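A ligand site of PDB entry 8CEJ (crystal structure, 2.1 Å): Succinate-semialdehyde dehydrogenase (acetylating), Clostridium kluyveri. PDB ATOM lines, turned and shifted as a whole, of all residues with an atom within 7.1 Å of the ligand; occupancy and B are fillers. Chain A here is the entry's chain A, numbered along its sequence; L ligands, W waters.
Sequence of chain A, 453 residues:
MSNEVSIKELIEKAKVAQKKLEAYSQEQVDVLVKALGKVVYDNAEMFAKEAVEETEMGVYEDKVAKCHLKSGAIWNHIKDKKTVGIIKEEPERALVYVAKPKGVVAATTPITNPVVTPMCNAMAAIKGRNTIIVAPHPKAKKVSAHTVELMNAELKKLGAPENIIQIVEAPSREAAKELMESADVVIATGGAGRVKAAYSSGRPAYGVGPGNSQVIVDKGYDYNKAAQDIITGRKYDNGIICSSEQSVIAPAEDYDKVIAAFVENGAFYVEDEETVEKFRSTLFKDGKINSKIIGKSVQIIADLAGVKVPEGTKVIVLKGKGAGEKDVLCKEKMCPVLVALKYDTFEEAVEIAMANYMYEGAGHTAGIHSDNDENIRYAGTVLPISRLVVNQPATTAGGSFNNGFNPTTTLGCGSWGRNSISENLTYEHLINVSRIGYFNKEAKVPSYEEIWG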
ATOM      1  N   LYS A  66      31.689 -14.229 -21.309  1.00  0.00           N
ATOM      2  CA  LYS A  66      31.160 -14.444 -22.646  1.00  0.00           C
ATOM      3  C   LYS A  66      30.860 -13.115 -23.339  1.00  0.00           C
ATOM      4  O   LYS A  66      31.214 -12.921 -24.501  1.00  0.00           O
ATOM      5  CB  LYS A  66      29.897 -15.305 -22.579  1.00  0.00           C
ATOM      6  CG  LYS A  66      29.323 -15.662 -23.933  1.00  0.00           C
ATOM      7  CD  LYS A  66      27.935 -16.275 -23.790  1.00  0.00           C
ATOM      8  CE  LYS A  66      27.967 -17.483 -22.880  1.00  0.00           C
ATOM      9  NZ  LYS A  66      26.604 -18.066 -22.717  1.00  0.00           N
ATOM     10  N   LEU A  69      34.258 -11.535 -24.098  1.00  0.00           N
ATOM     11  CA  LEU A  69      35.018 -12.219 -25.139  1.00  0.00           C
ATOM     12  C   LEU A  69      34.371 -12.037 -26.508  1.00  0.00           C
ATOM     13  O   LEU A  69      35.053 -11.695 -27.486  1.00  0.00           O
ATOM     14  CB  LEU A  69      35.167 -13.698 -24.800  1.00  0.00           C
ATOM     15  CG  LEU A  69      35.896 -14.560 -25.834  1.00  0.00           C
ATOM     16  CD1 LEU A  69      37.304 -14.055 -26.066  1.00  0.00           C
ATOM     17  CD2 LEU A  69      35.906 -16.020 -25.397  1.00  0.00           C
ATOM     18  N   LYS A  70      33.064 -12.278 -26.597  1.00  0.00           N
ATOM     19  CA  LYS A  70      32.388 -12.217 -27.894  1.00  0.00           C
ATOM     20  C   LYS A  70      32.417 -10.809 -28.465  1.00  0.00           C
ATOM     21  O   LYS A  70      32.736 -10.618 -29.653  1.00  0.00           O
ATOM     22  CB  LYS A  70      30.941 -12.705 -27.759  1.00  0.00           C
ATOM     23  CG  LYS A  70      30.815 -14.190 -27.448  1.00  0.00           C
ATOM     24  CD  LYS A  70      31.330 -15.047 -28.582  1.00  0.00           C
ATOM     25  CE  LYS A  70      31.137 -16.526 -28.283  1.00  0.00           C
ATOM     26  NZ  LYS A  70      31.605 -17.393 -29.397  1.00  0.00           N
ATOM     27  N   PRO A 110      18.687 -17.822 -29.339  1.00  0.00           N
ATOM     28  CA  PRO A 110      18.409 -18.923 -28.398  1.00  0.00           C
ATOM     29  C   PRO A 110      18.275 -18.473 -26.951  1.00  0.00           C
ATOM     30  O   PRO A 110      18.427 -17.291 -26.635  1.00  0.00           O
ATOM     31  CB  PRO A 110      19.624 -19.832 -28.578  1.00  0.00           C
ATOM     32  CG  PRO A 110      20.737 -18.879 -28.868  1.00  0.00           C
ATOM     33  CD  PRO A 110      20.121 -17.741 -29.667  1.00  0.00           C
ATOM     34  N   THR A 112      20.253 -19.909 -24.562  1.00  0.00           N
ATOM     35  CA  THR A 112      21.532 -20.143 -23.912  1.00  0.00           C
ATOM     36  C   THR A 112      22.446 -18.921 -24.009  1.00  0.00           C
ATOM     37  O   THR A 112      23.180 -18.618 -23.060  1.00  0.00           O
ATOM     38  CB  THR A 112      22.214 -21.367 -24.518  1.00  0.00           C
ATOM     39  OG1 THR A 112      22.281 -21.214 -25.947  1.00  0.00           O
ATOM     40  CG2 THR A 112      21.424 -22.619 -24.192  1.00  0.00           C
ATOM     41  N   ASN A 113      22.416 -18.222 -25.136  1.00  0.00           N
ATOM     42  CA  ASN A 113      23.222 -17.004 -25.344  1.00  0.00           C
ATOM     43  C   ASN A 113      22.302 -15.873 -25.765  1.00  0.00           C
ATOM     44  O   ASN A 113      22.392 -15.373 -26.894  1.00  0.00           O
ATOM     45  CB  ASN A 113      24.316 -17.241 -26.381  1.00  0.00           C
ATOM     46  CG  ASN A 113      25.127 -18.495 -26.090  1.00  0.00           C
ATOM     47  OD1 ASN A 113      25.943 -18.525 -25.170  1.00  0.00           O
ATOM     48  ND2 ASN A 113      24.920 -19.533 -26.898  1.00  0.00           N
ATOM     49  N   VAL A 116      24.730 -12.214 -26.368  1.00  0.00           N
ATOM     50  CA  VAL A 116      25.778 -12.099 -27.376  1.00  0.00           C
ATOM     51  C   VAL A 116      25.285 -12.492 -28.761  1.00  0.00           C
ATOM     52  O   VAL A 116      25.850 -12.051 -29.768  1.00  0.00           O
ATOM     53  CB  VAL A 116      27.001 -12.948 -26.985  1.00  0.00           C
ATOM     54  CG1 VAL A 116      27.684 -12.345 -25.764  1.00  0.00           C
ATOM     55  CG2 VAL A 116      26.592 -14.382 -26.716  1.00  0.00           C
ATOM     56  N   THR A 117      24.231 -13.319 -28.855  1.00  0.00           N
ATOM     57  CA  THR A 117      23.731 -13.696 -30.171  1.00  0.00           C
ATOM     58  C   THR A 117      22.981 -12.544 -30.842  1.00  0.00           C
ATOM     59  O   THR A 117      23.246 -12.271 -32.028  1.00  0.00           O
ATOM     60  CB  THR A 117      22.860 -14.957 -30.072  1.00  0.00           C
ATOM     61  OG1 THR A 117      23.651 -16.021 -29.531  1.00  0.00           O
ATOM     62  CG2 THR A 117      22.341 -15.359 -31.432  1.00  0.00           C
ATOM     63  N   THR A 189      19.536 -19.559 -34.774  1.00  0.00           N
ATOM     64  CA  THR A 189      20.426 -20.077 -33.729  1.00  0.00           C
ATOM     65  C   THR A 189      19.560 -20.625 -32.610  1.00  0.00           C
ATOM     66  O   THR A 189      18.986 -19.869 -31.820  1.00  0.00           O
ATOM     67  CB  THR A 189      21.363 -18.980 -33.219  1.00  0.00           C
ATOM     68  OG1 THR A 189      22.048 -18.381 -34.328  1.00  0.00           O
ATOM     69  CG2 THR A 189      22.386 -19.561 -32.260  1.00  0.00           C
ATOM     70  N   VAL A 208      22.229 -23.555 -37.311  1.00  0.00           N
ATOM     71  CA  VAL A 208      23.194 -24.249 -36.478  1.00  0.00           C
ATOM     72  C   VAL A 208      22.767 -25.703 -36.379  1.00  0.00           C
ATOM     73  O   VAL A 208      21.907 -26.164 -37.130  1.00  0.00           O
ATOM     74  CB  VAL A 208      23.310 -23.603 -35.091  1.00  0.00           C
ATOM     75  CG1 VAL A 208      23.862 -22.188 -35.201  1.00  0.00           C
ATOM     76  CG2 VAL A 208      21.954 -23.602 -34.400  1.00  0.00           C
ATOM     77  N   TYR A 236      31.747 -24.595 -18.393  1.00  0.00           N
ATOM     78  CA  TYR A 236      31.531 -23.228 -18.844  1.00  0.00           C
ATOM     79  C   TYR A 236      30.036 -22.958 -19.000  1.00  0.00           C
ATOM     80  O   TYR A 236      29.349 -23.630 -19.774  1.00  0.00           O
ATOM     81  CB  TYR A 236      32.253 -23.003 -20.166  1.00  0.00           C
ATOM     82  CG  TYR A 236      32.276 -21.566 -20.650  1.00  0.00           C
ATOM     83  CD1 TYR A 236      32.940 -20.586 -19.924  1.00  0.00           C
ATOM     84  CD2 TYR A 236      31.674 -21.208 -21.842  1.00  0.00           C
ATOM     85  CE1 TYR A 236      32.972 -19.275 -20.372  1.00  0.00           C
ATOM     86  CE2 TYR A 236      31.699 -19.909 -22.295  1.00  0.00           C
ATOM     87  CZ  TYR A 236      32.349 -18.943 -21.549  1.00  0.00           C
ATOM     88  OH  TYR A 236      32.383 -17.641 -22.003  1.00  0.00           O
ATOM     89  N   ILE A 240      26.037 -25.254 -21.192  1.00  0.00           N
ATOM     90  CA  ILE A 240      25.021 -25.015 -22.210  1.00  0.00           C
ATOM     91  C   ILE A 240      25.609 -24.580 -23.533  1.00  0.00           C
ATOM     92  O   ILE A 240      24.870 -24.412 -24.518  1.00  0.00           O
ATOM     93  CB  ILE A 240      23.970 -23.991 -21.734  1.00  0.00           C
ATOM     94  CG1 ILE A 240      24.654 -22.712 -21.239  1.00  0.00           C
ATOM     95  CG2 ILE A 240      23.091 -24.585 -20.660  1.00  0.00           C
ATOM     96  CD1 ILE A 240      23.689 -21.659 -20.760  1.00  0.00           C
ATOM     97  N   ILE A 241      26.926 -24.379 -23.609  1.00  0.00           N
ATOM     98  CA  ILE A 241      27.581 -23.993 -24.848  1.00  0.00           C
ATOM     99  C   ILE A 241      27.553 -25.157 -25.837  1.00  0.00           C
ATOM    100  O   ILE A 241      27.868 -26.294 -25.478  1.00  0.00           O
ATOM    101  CB  ILE A 241      29.016 -23.496 -24.587  1.00  0.00           C
ATOM    102  CG1 ILE A 241      28.983 -22.073 -24.028  1.00  0.00           C
ATOM    103  CG2 ILE A 241      29.853 -23.569 -25.848  1.00  0.00           C
ATOM    104  CD1 ILE A 241      28.411 -21.058 -25.001  1.00  0.00           C
ATOM    105  N   CYS A 242      27.166 -24.870 -27.073  1.00  0.00           N
ATOM    106  CA  CYS A 242      26.977 -25.887 -28.087  1.00  0.00           C
ATOM    107  C   CYS A 242      28.269 -26.631 -28.435  1.00  0.00           C
ATOM    108  O   CYS A 242      28.232 -27.833 -28.795  1.00  0.00           O
ATOM    109  CB  CYS A 242      26.384 -25.220 -29.337  1.00  0.00           C
ATOM    110  SG  CYS A 242      27.562 -24.011 -29.989  1.00  0.00           S
ATOM    111  N   SER A 243      29.411 -25.953 -28.319  1.00  0.00           N
ATOM    112  CA  SER A 243      30.691 -26.551 -28.677  1.00  0.00           C
ATOM    113  C   SER A 243      31.396 -27.156 -27.473  1.00  0.00           C
ATOM    114  O   SER A 243      32.513 -27.655 -27.578  1.00  0.00           O
ATOM    115  CB  SER A 243      31.590 -25.504 -29.335  1.00  0.00           C
ATOM    116  OG  SER A 243      31.782 -24.390 -28.480  1.00  0.00           O
ATOM    117  N   SER A 244      30.732 -27.114 -26.316  1.00  0.00           N
ATOM    118  CA  SER A 244      31.332 -27.593 -25.083  1.00  0.00           C
ATOM    119  C   SER A 244      31.629 -29.083 -25.146  1.00  0.00           C
ATOM    120  O   SER A 244      30.932 -29.854 -25.819  1.00  0.00           O
ATOM    121  CB  SER A 244      30.408 -27.291 -23.896  1.00  0.00           C
ATOM    122  OG  SER A 244      30.998 -27.706 -22.673  1.00  0.00           O
ATOM    123  N   HIS A 364      29.484 -30.586 -36.064  1.00  0.00           N
ATOM    124  CA  HIS A 364      29.775 -29.445 -35.200  1.00  0.00           C
ATOM    125  C   HIS A 364      31.255 -29.357 -34.857  1.00  0.00           C
ATOM    126  O   HIS A 364      32.069 -28.979 -35.712  1.00  0.00           O
ATOM    127  CB  HIS A 364      28.941 -29.517 -33.914  1.00  0.00           C
ATOM    128  CG  HIS A 364      28.719 -28.192 -33.258  1.00  0.00           C
ATOM    129  ND1 HIS A 364      29.762 -27.410 -32.798  1.00  0.00           N
ATOM    130  CD2 HIS A 364      27.589 -27.503 -32.999  1.00  0.00           C
ATOM    131  CE1 HIS A 364      29.268 -26.294 -32.281  1.00  0.00           C
ATOM    132  NE2 HIS A 364      27.953 -26.336 -32.389  1.00  0.00           N
ATOM    133  N   THR A 365      31.613 -29.693 -33.628  1.00  0.00           N
ATOM    134  CA  THR A 365      32.956 -29.451 -33.114  1.00  0.00           C
ATOM    135  C   THR A 365      33.513 -30.710 -32.469  1.00  0.00           C
ATOM    136  O   THR A 365      32.777 -31.532 -31.913  1.00  0.00           O
ATOM    137  CB  THR A 365      32.943 -28.302 -32.074  1.00  0.00           C
ATOM    138  OG1 THR A 365      32.256 -27.170 -32.633  1.00  0.00           O
ATOM    139  CG2 THR A 365      34.355 -27.891 -31.700  1.00  0.00           C
ATOM    140  N   ALA A 394      37.362 -26.814 -26.025  1.00  0.00           N
ATOM    141  CA  ALA A 394      36.551 -26.829 -27.242  1.00  0.00           C
ATOM    142  C   ALA A 394      35.583 -25.660 -27.310  1.00  0.00           C
ATOM    143  O   ALA A 394      35.118 -25.323 -28.401  1.00  0.00           O
ATOM    144  CB  ALA A 394      35.782 -28.143 -27.355  1.00  0.00           C
ATOM    145  N   THR A 395      35.271 -25.026 -26.169  1.00  0.00           N
ATOM    146  CA  THR A 395      34.408 -23.856 -26.162  1.00  0.00           C
ATOM    147  C   THR A 395      35.015 -22.655 -26.862  1.00  0.00           C
ATOM    148  O   THR A 395      34.308 -21.669 -27.106  1.00  0.00           O
ATOM    149  CB  THR A 395      34.043 -23.484 -24.724  1.00  0.00           C
ATOM    150  OG1 THR A 395      35.233 -23.381 -23.936  1.00  0.00           O
ATOM    151  CG2 THR A 395      33.116 -24.530 -24.117  1.00  0.00           C
ATOM    152  N   THR A 396      36.310 -22.710 -27.189  1.00  0.00           N
ATOM    153  CA  THR A 396      36.947 -21.648 -27.961  1.00  0.00           C
ATOM    154  C   THR A 396      36.685 -21.763 -29.451  1.00  0.00           C
ATOM    155  O   THR A 396      37.206 -20.952 -30.221  1.00  0.00           O
ATOM    156  CB  THR A 396      38.466 -21.663 -27.709  1.00  0.00           C
ATOM    157  OG1 THR A 396      39.027 -22.870 -28.247  1.00  0.00           O
ATOM    158  CG2 THR A 396      38.760 -21.585 -26.225  1.00  0.00           C
ATOM    159  N   ALA A 397      35.872 -22.744 -29.876  1.00  0.00           N
ATOM    160  CA  ALA A 397      35.597 -22.929 -31.294  1.00  0.00           C
ATOM    161  C   ALA A 397      34.830 -21.755 -31.889  1.00  0.00           C
ATOM    162  O   ALA A 397      34.827 -21.595 -33.118  1.00  0.00           O
ATOM    163  CB  ALA A 397      34.806 -24.217 -31.516  1.00  0.00           C
ATOM    164  N   GLY A 398      34.197 -20.925 -31.065  1.00  0.00           N
ATOM    165  CA  GLY A 398      33.493 -19.755 -31.515  1.00  0.00           C
ATOM    166  C   GLY A 398      34.346 -18.512 -31.630  1.00  0.00           C
ATOM    167  O   GLY A 398      33.800 -17.411 -31.753  1.00  0.00           O
ATOM    168  N   GLY A 399      35.671 -18.644 -31.584  1.00  0.00           N
ATOM    169  CA  GLY A 399      36.552 -17.499 -31.702  1.00  0.00           C
ATOM    170  C   GLY A 399      37.304 -17.184 -30.434  1.00  0.00           C
ATOM    171  O   GLY A 399      36.706 -17.014 -29.368  1.00  0.00           O
ATOM    172  N   THR A 408      32.260 -15.583 -33.482  1.00  0.00           N
ATOM    173  CA  THR A 408      30.834 -15.634 -33.809  1.00  0.00           C
ATOM    174  C   THR A 408      30.073 -16.182 -32.615  1.00  0.00           C
ATOM    175  O   THR A 408      30.660 -16.662 -31.637  1.00  0.00           O
ATOM    176  CB  THR A 408      30.563 -16.503 -35.037  1.00  0.00           C
ATOM    177  OG1 THR A 408      29.259 -16.198 -35.558  1.00  0.00           O
ATOM    178  CG2 THR A 408      30.610 -17.973 -34.650  1.00  0.00           C
ATOM    179  N   THR A 409      28.748 -16.107 -32.703  1.00  0.00           N
ATOM    180  CA  THR A 409      27.851 -16.844 -31.831  1.00  0.00           C
ATOM    181  C   THR A 409      27.027 -17.872 -32.594  1.00  0.00           C
ATOM    182  O   THR A 409      26.241 -18.600 -31.973  1.00  0.00           O
ATOM    183  CB  THR A 409      26.919 -15.887 -31.085  1.00  0.00           C
ATOM    184  OG1 THR A 409      26.104 -15.180 -32.025  1.00  0.00           O
ATOM    185  CG2 THR A 409      27.719 -14.890 -30.260  1.00  0.00           C
ATOM    186  N   THR A 410      27.171 -17.933 -33.916  1.00  0.00           N
ATOM    187  CA  THR A 410      26.414 -18.841 -34.775  1.00  0.00           C
ATOM    188  C   THR A 410      27.402 -19.778 -35.456  1.00  0.00           C
ATOM    189  O   THR A 410      28.065 -19.402 -36.421  1.00  0.00           O
ATOM    190  CB  THR A 410      25.595 -18.049 -35.797  1.00  0.00           C
ATOM    191  OG1 THR A 410      24.739 -17.131 -35.118  1.00  0.00           O
ATOM    192  CG2 THR A 410      24.755 -18.990 -36.650  1.00  0.00           C
ATOM    193  N   LEU A 411      27.499 -21.001 -34.951  1.00  0.00           N
ATOM    194  CA  LEU A 411      28.432 -22.000 -35.473  1.00  0.00           C
ATOM    195  C   LEU A 411      27.682 -22.936 -36.420  1.00  0.00           C
ATOM    196  O   LEU A 411      26.866 -23.752 -35.978  1.00  0.00           O
ATOM    197  CB  LEU A 411      29.088 -22.790 -34.332  1.00  0.00           C
ATOM    198  CG  LEU A 411      30.211 -22.125 -33.535  1.00  0.00           C
ATOM    199  CD1 LEU A 411      29.684 -21.035 -32.612  1.00  0.00           C
ATOM    200  CD2 LEU A 411      30.985 -23.158 -32.736  1.00  0.00           C
ATOM    201  N   ASN A 424      31.950 -20.854 -39.065  1.00  0.00           N
ATOM    202  CA  ASN A 424      31.382 -19.832 -38.202  1.00  0.00           C
ATOM    203  C   ASN A 424      30.749 -18.724 -39.036  1.00  0.00           C
ATOM    204  O   ASN A 424      31.280 -18.326 -40.080  1.00  0.00           O
ATOM    205  CB  ASN A 424      32.455 -19.264 -37.279  1.00  0.00           C
ATOM    206  CG  ASN A 424      32.885 -20.248 -36.212  1.00  0.00           C
ATOM    207  OD1 ASN A 424      32.579 -21.440 -36.288  1.00  0.00           O
ATOM    208  ND2 ASN A 424      33.583 -19.755 -35.196  1.00  0.00           N
HETATM  209  O1  LIG L   1      26.210 -22.113 -28.784  1.00  0.00           O
HETATM  210  C1  LIG L   1      27.277 -22.381 -29.230  1.00  0.00           C
HETATM  211  C2  LIG L   1      28.412 -21.371 -29.155  1.00  0.00           C
HETATM  212  C3  LIG L   1      28.151 -19.908 -29.506  1.00  0.00           C
HETATM  213  C4  LIG L   1      29.612 -21.787 -28.781  1.00  0.00           C
HETATM  214  C5  LIG L   1      30.838 -20.891 -28.664  1.00  0.00           C
HETATM  215  O2  LIG L   1      30.815 -19.834 -27.966  1.00  0.00           O
HETATM  216  O3  LIG L   1      31.901 -21.214 -29.257  1.00  0.00           O
HETATM  217  O   HOH W   1      23.818 -21.444 -29.201  1.00  0.00           O
HETATM  218  O   HOH W   2      24.645 -22.539 -26.830  1.00  0.00           O
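An oxygen (O1) of the ligand sits close to the backbone NH (N) of Cys 242.
The backbone NH (N) of Gly 398 sits at hydrogen-bond distance from an oxygen (O3) of the ligand (2.9 Å).
SG of Cys 242 is covalently linked to C1 of the ligand (1.8 Å).
O2 of the ligand lies within salt-bridge range of NZ of Lys 70.
The side-chain hydroxyl (OG) of Ser 243 sits at hydrogen-bond distance from an oxygen (O3) of the ligand, at 3.3 Å.
The side-chain amide nitrogen (ND2) of Asn 113 sits at hydrogen-bond distance from an oxygen (O1) of the ligand, 3.4 Å away.
A ring nitrogen (NE2) of His 364 lies within hydrogen-bond range of the side-chain sulfur of Cys 242 (3.4 Å).
O of Ala 397 sits at hydrogen-bond distance from ND2 of Asn 424, at 3.0 Å.
OG of Ser 243 sits at hydrogen-bond distance from O of Ala 394 (3.5 Å).
The side-chain amino group of Lys 70 is in hydrogen-bond range of the backbone carbonyl oxygen of Gly 398, 3.2 Å away.
O of Thr 408 lies within hydrogen-bond range of NZ of Lys 70 (2.5 Å).
ND2 of Asn 113 sits at hydrogen-bond distance from OG1 of Thr 112, at 3.3 Å.
The backbone NH of Thr 408 sits at hydrogen-bond distance from the backbone carbonyl oxygen of Gly 398 (3.0 Å).
OG1 of Thr 117 sits at hydrogen-bond distance from O of Asn 113 (3.0 Å).
An oxygen (O3) of the ligand lies close to the backbone carbonyl oxygen (O) of Thr 395 (3.3 Å).
CG2 of Ile 241 touches C4 of the ligand, at 3.4 Å.
Ala 397 touches the ligand.
Thr 409 touches the ligand.
CD1 of Leu 411 touches C3 of the ligand (3.6 Å).
The nearest printed residue that does not touch the ligand is Thr 408 (4.6 Å).
Water W1 bridges an oxygen (O1) of the ligand and the side-chain amide nitrogen (ND2) of Asn 113.
Water W2 lies within hydrogen-bond range of O1 of the ligand, OG1 of Thr 112, O of Ile 240, ND2 of Asn 113 and N of Cys 242.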
